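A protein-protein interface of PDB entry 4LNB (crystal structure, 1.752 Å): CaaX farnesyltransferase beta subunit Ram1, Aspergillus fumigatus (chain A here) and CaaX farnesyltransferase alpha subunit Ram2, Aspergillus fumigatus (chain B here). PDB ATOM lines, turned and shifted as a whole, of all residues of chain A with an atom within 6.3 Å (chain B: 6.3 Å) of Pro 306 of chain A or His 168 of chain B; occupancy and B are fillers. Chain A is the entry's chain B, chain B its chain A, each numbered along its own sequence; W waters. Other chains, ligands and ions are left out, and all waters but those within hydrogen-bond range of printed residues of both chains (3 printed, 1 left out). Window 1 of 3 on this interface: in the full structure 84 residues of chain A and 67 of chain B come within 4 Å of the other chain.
NH1 of Arg 172 of chain B lies within salt-bridge range of OD1 of Asp 217 of chain B.
The backbone carbonyl oxygen (O) of Asp 238 of chain A lies within hydrogen-bond range of the guanidinium group (NH2) of Arg 294 of chain A.
The side-chain hydroxyl (OG) of Ser 303 of chain A is in hydrogen-bond range of the backbone carbonyl oxygen (O) of Ser 305 of chain A (2.7 Å).
OG of Ser 303 of chain A lies close to O of Ser 308 of chain A, 3.4 Å away.
The side-chain hydroxyl (OG) of Ser 305 of chain A sits at hydrogen-bond distance from the side-chain hydroxyl (OG) of Ser 308 of chain A.
Of the printed residues of chain B, Pro 306 of chain A touches His 168, Asp 217 and Ala 218.
Of the printed residues of chain A, His 168 of chain B touches Pro 306 (3.0 Å) and Gly 307 (3.4 Å).
Printed residues of chain B within 4 Å of Arg 294 of chain A: Asp 217, Ala 218 and Gly 219.
Of the printed residues of chain B, Gly 307 of chain A touches His 168 (3.4 Å), Asn 201 (3.1 Å) and Gly 219 (3.7 Å).
Of the printed residues of chain A, Asp 217 of chain B touches Arg 294 and Pro 306.
Val 171 of chain B touches none of the printed residues of chain A.
Trp 169 of chain B touches none of the printed residues of chain A.
The nearest printed residue of chain B that does not touch Pro 306 of chain A is Gly 219 of chain B (4.1 Å).
The nearest printed residue of chain A that does not touch Ala 218 of chain B is Gly 307 of chain A (4.3 Å).
OG1 of Thr 165 of chain B sits at hydrogen-bond distance from OG of Ser 308 of chain A.
The backbone carbonyl oxygen of Pro 306 of chain A lies close to a ring nitrogen (NE2) of His 168 of chain B, 3.4 Å away.
ND2 of Asn 201 of chain B is in hydrogen-bond range of O of Gly 307 of chain A, 3.1 Å away.
The guanidinium group (NE) of Arg 294 of chain A lies within hydrogen-bond range of the backbone carbonyl oxygen (O) of Asp 217 of chain B (3.1 Å).
The backbone carbonyl oxygen (O) of Arg 294 of chain A is in hydrogen-bond range of the backbone NH (N) of Gly 219 of chain B (3.0 Å).
Of the 17 printed residues of chain B, 6 touch a printed residue of chain A.
Hydrophobic or aromatic side chains of chain B within 4 Å of the printed part of chain A: His 168 and Ala 218.
Of the 11 printed residues of chain A, 5 touch a printed residue of chain B.
Printed residues of chain A that touch a printed residue of chain B: Arg 294, Ser 305, Pro 306, Gly 307 and Ser 308.
Hydrophobic or aromatic side chains of chain A that line the printed part of chain B: Pro 306.
Water W3 lies within hydrogen-bond range of OG of Ser 305 of chain A, OG of Ser 308 of chain A and OG1 of Thr 165 of chain B.
Water W1 lies within hydrogen-bond range of O of Asp 217 of chain B, NH2 of Arg 294 of chain A and OD2 of Asp 238 of chain A.
Water W2 bridges O of Asn 201 of chain B and O of Gly 307 of chain A.
Among the printed residues, pairs that only touch across the chains: Gly 307 of chain A with His 168 of chain B (3.4 Å), Ser 308 of chain A with Asn 201 of chain B (3.4 Å), Pro 306 of chain A with Asp 217 of chain B (3.5 Å), Arg 294 of chain A with Ala 218 of chain B (3.5 Å), Gly 307 of chain A with Gly 219 of chain B (3.7 Å), Pro 306 of chain A with Ala 218 of chain B (3.7 Å) and Ser 305 of chain A with Thr 165 of chain B (3.9 Å).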
ATOM      1  N   ASP A 238      14.770  -3.565  29.561  1.00  0.00           N
ATOM      2  CA  ASP A 238      14.025  -3.354  28.321  1.00  0.00           C
ATOM      3  C   ASP A 238      14.516  -2.138  27.526  1.00  0.00           C
ATOM      4  O   ASP A 238      13.963  -1.803  26.479  1.00  0.00           O
ATOM      5  CB  ASP A 238      12.512  -3.295  28.584  1.00  0.00           C
ATOM      6  CG  ASP A 238      12.065  -1.990  29.223  1.00  0.00           C
ATOM      7  OD1 ASP A 238      12.919  -1.207  29.686  1.00  0.00           O
ATOM      8  OD2 ASP A 238      10.839  -1.750  29.269  1.00  0.00           O
ATOM      9  N   GLU A 249       8.674   3.750  35.072  1.00  0.00           N
ATOM     10  CA  GLU A 249       9.427   3.766  33.825  1.00  0.00           C
ATOM     11  C   GLU A 249       8.552   4.302  32.699  1.00  0.00           C
ATOM     12  O   GLU A 249       7.559   3.679  32.322  1.00  0.00           O
ATOM     13  CB  GLU A 249       9.937   2.369  33.460  1.00  0.00           C
ATOM     14  CG  GLU A 249      10.622   2.350  32.100  1.00  0.00           C
ATOM     15  CD  GLU A 249      11.240   1.018  31.738  1.00  0.00           C
ATOM     16  OE1 GLU A 249      10.980   0.005  32.421  1.00  0.00           O
ATOM     17  OE2 GLU A 249      11.996   0.991  30.749  1.00  0.00           O
ATOM     18  N   TYR A 291      13.201   0.345  22.512  1.00  0.00           N
ATOM     19  CA  TYR A 291      12.198   0.657  23.521  1.00  0.00           C
ATOM     20  C   TYR A 291      11.245   1.754  23.042  1.00  0.00           C
ATOM     21  O   TYR A 291      10.026   1.626  23.156  1.00  0.00           O
ATOM     22  CB  TYR A 291      12.884   1.072  24.828  1.00  0.00           C
ATOM     23  CG  TYR A 291      11.980   1.765  25.821  1.00  0.00           C
ATOM     24  CD1 TYR A 291      11.115   1.039  26.633  1.00  0.00           C
ATOM     25  CD2 TYR A 291      12.004   3.147  25.962  1.00  0.00           C
ATOM     26  CE1 TYR A 291      10.293   1.676  27.548  1.00  0.00           C
ATOM     27  CE2 TYR A 291      11.187   3.788  26.865  1.00  0.00           C
ATOM     28  CZ  TYR A 291      10.338   3.051  27.658  1.00  0.00           C
ATOM     29  OH  TYR A 291       9.528   3.697  28.562  1.00  0.00           O
ATOM     30  N   ARG A 294       8.702   0.580  20.612  1.00  0.00           N
ATOM     31  CA  ARG A 294       7.619  -0.179  21.233  1.00  0.00           C
ATOM     32  C   ARG A 294       6.608   0.713  21.957  1.00  0.00           C
ATOM     33  O   ARG A 294       5.615   0.224  22.506  1.00  0.00           O
ATOM     34  CB  ARG A 294       8.181  -1.229  22.197  1.00  0.00           C
ATOM     35  CG  ARG A 294       9.094  -2.252  21.532  1.00  0.00           C
ATOM     36  CD  ARG A 294       9.373  -3.445  22.441  1.00  0.00           C
ATOM     37  NE  ARG A 294       9.990  -3.045  23.701  1.00  0.00           N
ATOM     38  CZ  ARG A 294      11.301  -2.928  23.890  1.00  0.00           C
ATOM     39  NH1 ARG A 294      12.145  -3.180  22.897  1.00  0.00           N
ATOM     40  NH2 ARG A 294      11.768  -2.556  25.073  1.00  0.00           N
ATOM     41  N   CYS A 295       6.862   2.017  21.959  1.00  0.00           N
ATOM     42  CA  CYS A 295       5.920   2.972  22.534  1.00  0.00           C
ATOM     43  C   CYS A 295       5.030   3.626  21.479  1.00  0.00           C
ATOM     44  O   CYS A 295       4.126   4.392  21.814  1.00  0.00           O
ATOM     45  CB  CYS A 295       6.653   4.041  23.352  1.00  0.00           C
ATOM     46  SG  CYS A 295       7.343   3.415  24.906  1.00  0.00           S
ATOM     47  N   SER A 303       3.133   6.746  23.155  1.00  0.00           N
ATOM     48  CA  SER A 303       2.601   6.726  24.514  1.00  0.00           C
ATOM     49  C   SER A 303       3.705   6.804  25.570  1.00  0.00           C
ATOM     50  O   SER A 303       4.890   6.717  25.250  1.00  0.00           O
ATOM     51  CB  SER A 303       1.777   5.461  24.730  1.00  0.00           C
ATOM     52  OG  SER A 303       2.565   4.294  24.549  1.00  0.00           O
ATOM     53  N   GLY A 304       3.309   6.962  26.829  1.00  0.00           N
ATOM     54  CA  GLY A 304       4.265   7.061  27.919  1.00  0.00           C
ATOM     55  C   GLY A 304       5.006   5.773  28.192  1.00  0.00           C
ATOM     56  O   GLY A 304       6.180   5.781  28.560  1.00  0.00           O
ATOM     57  N   SER A 305       4.304   4.661  28.020  1.00  0.00           N
ATOM     58  CA  SER A 305       4.887   3.334  28.164  1.00  0.00           C
ATOM     59  C   SER A 305       4.169   2.437  27.159  1.00  0.00           C
ATOM     60  O   SER A 305       3.093   2.800  26.679  1.00  0.00           O
ATOM     61  CB  SER A 305       4.730   2.830  29.605  1.00  0.00           C
ATOM     62  OG  SER A 305       3.420   3.047  30.099  1.00  0.00           O
ATOM     63  N   PRO A 306       4.771   1.287  26.807  1.00  0.00           N
ATOM     64  CA  PRO A 306       4.167   0.413  25.789  1.00  0.00           C
ATOM     65  C   PRO A 306       2.710   0.064  26.081  1.00  0.00           C
ATOM     66  O   PRO A 306       2.387  -0.380  27.182  1.00  0.00           O
ATOM     67  CB  PRO A 306       5.038  -0.841  25.858  1.00  0.00           C
ATOM     68  CG  PRO A 306       6.376  -0.324  26.250  1.00  0.00           C
ATOM     69  CD  PRO A 306       6.105   0.810  27.213  1.00  0.00           C
ATOM     70  N   GLY A 307       1.839   0.290  25.101  1.00  0.00           N
ATOM     71  CA  GLY A 307       0.438  -0.069  25.231  1.00  0.00           C
ATOM     72  C   GLY A 307      -0.474   1.060  25.674  1.00  0.00           C
ATOM     73  O   GLY A 307      -1.692   0.980  25.508  1.00  0.00           O
ATOM     74  N   SER A 308       0.102   2.113  26.250  1.00  0.00           N
ATOM     75  CA  SER A 308      -0.698   3.246  26.700  1.00  0.00           C
ATOM     76  C   SER A 308      -1.169   4.099  25.520  1.00  0.00           C
ATOM     77  O   SER A 308      -0.843   3.819  24.367  1.00  0.00           O
ATOM     78  CB  SER A 308       0.071   4.092  27.718  1.00  0.00           C
ATOM     79  OG  SER A 308       0.146   3.420  28.966  1.00  0.00           O
ATOM     80  N   VAL B 163      -4.816   6.013  35.423  1.00  0.00           N
ATOM     81  CA  VAL B 163      -5.646   4.855  35.730  1.00  0.00           C
ATOM     82  C   VAL B 163      -5.682   3.889  34.541  1.00  0.00           C
ATOM     83  O   VAL B 163      -5.602   2.672  34.720  1.00  0.00           O
ATOM     84  CB  VAL B 163      -7.077   5.246  36.178  1.00  0.00           C
ATOM     85  CG1 VAL B 163      -7.883   3.997  36.527  1.00  0.00           C
ATOM     86  CG2 VAL B 163      -7.019   6.169  37.386  1.00  0.00           C
ATOM     87  N   TRP B 164      -5.788   4.428  33.330  1.00  0.00           N
ATOM     88  CA  TRP B 164      -5.737   3.581  32.138  1.00  0.00           C
ATOM     89  C   TRP B 164      -4.389   2.871  32.009  1.00  0.00           C
ATOM     90  O   TRP B 164      -4.333   1.695  31.647  1.00  0.00           O
ATOM     91  CB  TRP B 164      -6.041   4.387  30.872  1.00  0.00           C
ATOM     92  CG  TRP B 164      -7.509   4.631  30.658  1.00  0.00           C
ATOM     93  CD1 TRP B 164      -8.171   5.821  30.778  1.00  0.00           C
ATOM     94  CD2 TRP B 164      -8.499   3.656  30.293  1.00  0.00           C
ATOM     95  NE1 TRP B 164      -9.508   5.648  30.509  1.00  0.00           N
ATOM     96  CE2 TRP B 164      -9.736   4.330  30.207  1.00  0.00           C
ATOM     97  CE3 TRP B 164      -8.458   2.282  30.025  1.00  0.00           C
ATOM     98  CZ2 TRP B 164     -10.923   3.677  29.858  1.00  0.00           C
ATOM     99  CZ3 TRP B 164      -9.641   1.632  29.686  1.00  0.00           C
ATOM    100  CH2 TRP B 164     -10.855   2.330  29.607  1.00  0.00           C
ATOM    101  N   THR B 165      -3.310   3.588  32.300  1.00  0.00           N
ATOM    102  CA  THR B 165      -1.973   2.999  32.259  1.00  0.00           C
ATOM    103  C   THR B 165      -1.865   1.860  33.271  1.00  0.00           C
ATOM    104  O   THR B 165      -1.301   0.800  32.978  1.00  0.00           O
ATOM    105  CB  THR B 165      -0.885   4.055  32.538  1.00  0.00           C
ATOM    106  OG1 THR B 165      -0.868   5.021  31.476  1.00  0.00           O
ATOM    107  CG2 THR B 165       0.486   3.402  32.643  1.00  0.00           C
ATOM    108  N   TYR B 166      -2.418   2.073  34.460  1.00  0.00           N
ATOM    109  CA  TYR B 166      -2.436   1.016  35.464  1.00  0.00           C
ATOM    110  C   TYR B 166      -3.242  -0.181  34.966  1.00  0.00           C
ATOM    111  O   TYR B 166      -2.848  -1.328  35.169  1.00  0.00           O
ATOM    112  CB  TYR B 166      -2.999   1.514  36.798  1.00  0.00           C
ATOM    113  CG  TYR B 166      -3.190   0.397  37.806  1.00  0.00           C
ATOM    114  CD1 TYR B 166      -2.118  -0.096  38.540  1.00  0.00           C
ATOM    115  CD2 TYR B 166      -4.441  -0.176  38.007  1.00  0.00           C
ATOM    116  CE1 TYR B 166      -2.288  -1.127  39.447  1.00  0.00           C
ATOM    117  CE2 TYR B 166      -4.623  -1.204  38.910  1.00  0.00           C
ATOM    118  CZ  TYR B 166      -3.544  -1.673  39.631  1.00  0.00           C
ATOM    119  OH  TYR B 166      -3.731  -2.696  40.536  1.00  0.00           O
ATOM    120  N   ARG B 167      -4.374   0.084  34.321  1.00  0.00           N
ATOM    121  CA  ARG B 167      -5.221  -1.006  33.849  1.00  0.00           C
ATOM    122  C   ARG B 167      -4.521  -1.813  32.758  1.00  0.00           C
ATOM    123  O   ARG B 167      -4.686  -3.026  32.687  1.00  0.00           O
ATOM    124  CB  ARG B 167      -6.594  -0.510  33.376  1.00  0.00           C
ATOM    125  CG  ARG B 167      -7.567  -1.666  33.107  1.00  0.00           C
ATOM    126  CD  ARG B 167      -9.040  -1.257  33.131  1.00  0.00           C
ATOM    127  NE  ARG B 167      -9.891  -2.439  33.269  1.00  0.00           N
ATOM    128  CZ  ARG B 167     -11.158  -2.420  33.674  1.00  0.00           C
ATOM    129  NH1 ARG B 167     -11.748  -1.272  33.981  1.00  0.00           N
ATOM    130  NH2 ARG B 167     -11.836  -3.558  33.773  1.00  0.00           N
ATOM    131  N   HIS B 168      -3.736  -1.144  31.912  1.00  0.00           N
ATOM    132  CA  HIS B 168      -2.962  -1.854  30.906  1.00  0.00           C
ATOM    133  C   HIS B 168      -1.986  -2.813  31.577  1.00  0.00           C
ATOM    134  O   HIS B 168      -1.886  -3.984  31.193  1.00  0.00           O
ATOM    135  CB  HIS B 168      -2.191  -0.889  30.009  1.00  0.00           C
ATOM    136  CG  HIS B 168      -1.253  -1.576  29.068  1.00  0.00           C
ATOM    137  ND1 HIS B 168       0.033  -1.926  29.422  1.00  0.00           N
ATOM    138  CD2 HIS B 168      -1.418  -1.993  27.791  1.00  0.00           C
ATOM    139  CE1 HIS B 168       0.619  -2.526  28.402  1.00  0.00           C
ATOM    140  NE2 HIS B 168      -0.239  -2.578  27.400  1.00  0.00           N
ATOM    141  N   TRP B 169      -1.280  -2.315  32.586  1.00  0.00           N
ATOM    142  CA  TRP B 169      -0.326  -3.127  33.327  1.00  0.00           C
ATOM    143  C   TRP B 169      -1.030  -4.316  33.971  1.00  0.00           C
ATOM    144  O   TRP B 169      -0.528  -5.441  33.941  1.00  0.00           O
ATOM    145  CB  TRP B 169       0.390  -2.295  34.395  1.00  0.00           C
ATOM    146  CG  TRP B 169       1.200  -3.156  35.305  1.00  0.00           C
ATOM    147  CD1 TRP B 169       2.491  -3.558  35.121  1.00  0.00           C
ATOM    148  CD2 TRP B 169       0.758  -3.770  36.521  1.00  0.00           C
ATOM    149  NE1 TRP B 169       2.884  -4.371  36.155  1.00  0.00           N
ATOM    150  CE2 TRP B 169       1.839  -4.515  37.029  1.00  0.00           C
ATOM    151  CE3 TRP B 169      -0.444  -3.751  37.235  1.00  0.00           C
ATOM    152  CZ2 TRP B 169       1.755  -5.238  38.217  1.00  0.00           C
ATOM    153  CZ3 TRP B 169      -0.527  -4.471  38.413  1.00  0.00           C
ATOM    154  CH2 TRP B 169       0.567  -5.204  38.893  1.00  0.00           C
ATOM    155  N   LEU B 170      -2.200  -4.054  34.546  1.00  0.00           N
ATOM    156  CA  LEU B 170      -2.978  -5.078  35.230  1.00  0.00           C
ATOM    157  C   LEU B 170      -3.356  -6.213  34.287  1.00  0.00           C
ATOM    158  O   LEU B 170      -3.273  -7.388  34.644  1.00  0.00           O
ATOM    159  CB  LEU B 170      -4.241  -4.461  35.835  1.00  0.00           C
ATOM    160  CG  LEU B 170      -5.047  -5.351  36.777  1.00  0.00           C
ATOM    161  CD1 LEU B 170      -4.304  -5.541  38.098  1.00  0.00           C
ATOM    162  CD2 LEU B 170      -6.431  -4.753  37.004  1.00  0.00           C
ATOM    163  N   VAL B 171      -3.769  -5.855  33.075  1.00  0.00           N
ATOM    164  CA  VAL B 171      -4.154  -6.852  32.085  1.00  0.00           C
ATOM    165  C   VAL B 171      -2.970  -7.743  31.718  1.00  0.00           C
ATOM    166  O   VAL B 171      -3.104  -8.963  31.629  1.00  0.00           O
ATOM    167  CB  VAL B 171      -4.729  -6.195  30.818  1.00  0.00           C
ATOM    168  CG1 VAL B 171      -4.880  -7.225  29.700  1.00  0.00           C
ATOM    169  CG2 VAL B 171      -6.068  -5.537  31.126  1.00  0.00           C
ATOM    170  N   ARG B 172      -1.810  -7.131  31.518  1.00  0.00           N
ATOM    171  CA  ARG B 172      -0.615  -7.889  31.161  1.00  0.00           C
ATOM    172  C   ARG B 172      -0.149  -8.777  32.313  1.00  0.00           C
ATOM    173  O   ARG B 172       0.216  -9.937  32.111  1.00  0.00           O
ATOM    174  CB  ARG B 172       0.508  -6.944  30.733  1.00  0.00           C
ATOM    175  CG  ARG B 172       1.762  -7.651  30.255  1.00  0.00           C
ATOM    176  CD  ARG B 172       2.757  -6.672  29.654  1.00  0.00           C
ATOM    177  NE  ARG B 172       3.938  -7.356  29.137  1.00  0.00           N
ATOM    178  CZ  ARG B 172       4.013  -7.908  27.930  1.00  0.00           C
ATOM    179  NH1 ARG B 172       2.972  -7.859  27.109  1.00  0.00           N
ATOM    180  NH2 ARG B 172       5.129  -8.510  27.544  1.00  0.00           N
ATOM    181  N   HIS B 173      -0.178  -8.227  33.522  1.00  0.00           N
ATOM    182  CA  HIS B 173       0.324  -8.922  34.700  1.00  0.00           C
ATOM    183  C   HIS B 173      -0.489 -10.173  35.028  1.00  0.00           C
ATOM    184  O   HIS B 173       0.074 -11.238  35.282  1.00  0.00           O
ATOM    185  CB  HIS B 173       0.344  -7.979  35.904  1.00  0.00           C
ATOM    186  CG  HIS B 173       0.936  -8.588  37.138  1.00  0.00           C
ATOM    187  ND1 HIS B 173       2.294  -8.739  37.314  1.00  0.00           N
ATOM    188  CD2 HIS B 173       0.353  -9.088  38.252  1.00  0.00           C
ATOM    189  CE1 HIS B 173       2.523  -9.307  38.486  1.00  0.00           C
ATOM    190  NE2 HIS B 173       1.363  -9.529  39.075  1.00  0.00           N
ATOM    191  N   ASN B 201      -8.344   2.748  22.843  1.00  0.00           N
ATOM    192  CA  ASN B 201      -6.952   2.326  22.921  1.00  0.00           C
ATOM    193  C   ASN B 201      -6.807   1.039  23.727  1.00  0.00           C
ATOM    194  O   ASN B 201      -6.044   0.146  23.358  1.00  0.00           O
ATOM    195  CB  ASN B 201      -6.084   3.433  23.520  1.00  0.00           C
ATOM    196  CG  ASN B 201      -4.628   3.033  23.623  1.00  0.00           C
ATOM    197  OD1 ASN B 201      -3.913   3.004  22.624  1.00  0.00           O
ATOM    198  ND2 ASN B 201      -4.185   2.712  24.833  1.00  0.00           N
ATOM    199  N   HIS B 202      -7.551   0.946  24.825  1.00  0.00           N
ATOM    200  CA  HIS B 202      -7.515  -0.248  25.665  1.00  0.00           C
ATOM    201  C   HIS B 202      -8.089  -1.427  24.897  1.00  0.00           C
ATOM    202  O   HIS B 202      -7.603  -2.553  25.017  1.00  0.00           O
ATOM    203  CB  HIS B 202      -8.307  -0.027  26.955  1.00  0.00           C
ATOM    204  CG  HIS B 202      -8.103  -1.096  27.988  1.00  0.00           C
ATOM    205  ND1 HIS B 202      -6.924  -1.243  28.686  1.00  0.00           N
ATOM    206  CD2 HIS B 202      -8.936  -2.057  28.452  1.00  0.00           C
ATOM    207  CE1 HIS B 202      -7.040  -2.249  29.536  1.00  0.00           C
ATOM    208  NE2 HIS B 202      -8.249  -2.764  29.409  1.00  0.00           N
ATOM    209  N   MET B 205      -5.494  -2.947  22.714  1.00  0.00           N
ATOM    210  CA  MET B 205      -4.578  -3.789  23.474  1.00  0.00           C
ATOM    211  C   MET B 205      -5.199  -5.157  23.752  1.00  0.00           C
ATOM    212  O   MET B 205      -4.547  -6.188  23.587  1.00  0.00           O
ATOM    213  CB  MET B 205      -4.164  -3.105  24.774  1.00  0.00           C
ATOM    214  CG  MET B 205      -3.159  -3.908  25.581  1.00  0.00           C
ATOM    215  SD  MET B 205      -3.961  -4.842  26.891  1.00  0.00           S
ATOM    216  CE  MET B 205      -4.474  -3.507  27.947  1.00  0.00           C
ATOM    217  N   ASP B 217       7.340  -5.719  26.504  1.00  0.00           N
ATOM    218  CA  ASP B 217       6.018  -5.202  26.165  1.00  0.00           C
ATOM    219  C   ASP B 217       6.104  -4.197  25.019  1.00  0.00           C
ATOM    220  O   ASP B 217       7.106  -3.499  24.868  1.00  0.00           O
ATOM    221  CB  ASP B 217       5.365  -4.558  27.390  1.00  0.00           C
ATOM    222  CG  ASP B 217       3.867  -4.367  27.222  1.00  0.00           C
ATOM    223  OD1 ASP B 217       3.294  -4.894  26.242  1.00  0.00           O
ATOM    224  OD2 ASP B 217       3.259  -3.698  28.084  1.00  0.00           O
ATOM    225  N   ALA B 218       5.050  -4.135  24.214  1.00  0.00           N
ATOM    226  CA  ALA B 218       5.005  -3.225  23.077  1.00  0.00           C
ATOM    227  C   ALA B 218       3.556  -2.868  22.776  1.00  0.00           C
ATOM    228  O   ALA B 218       2.651  -3.647  23.063  1.00  0.00           O
ATOM    229  CB  ALA B 218       5.660  -3.867  21.861  1.00  0.00           C
ATOM    230  N   GLY B 219       3.334  -1.689  22.210  1.00  0.00           N
ATOM    231  CA  GLY B 219       1.994  -1.296  21.816  1.00  0.00           C
ATOM    232  C   GLY B 219       1.560  -2.011  20.550  1.00  0.00           C
ATOM    233  O   GLY B 219       0.367  -2.195  20.301  1.00  0.00           O
HETATM  234  O   HOH W   1       9.217  -2.599  26.662  1.00  0.00           O
HETATM  235  O   HOH W   2      -3.071  -0.277  23.072  1.00  0.00           O
HETATM  236  O   HOH W   3       2.061   5.369  30.198  1.00  0.00           O
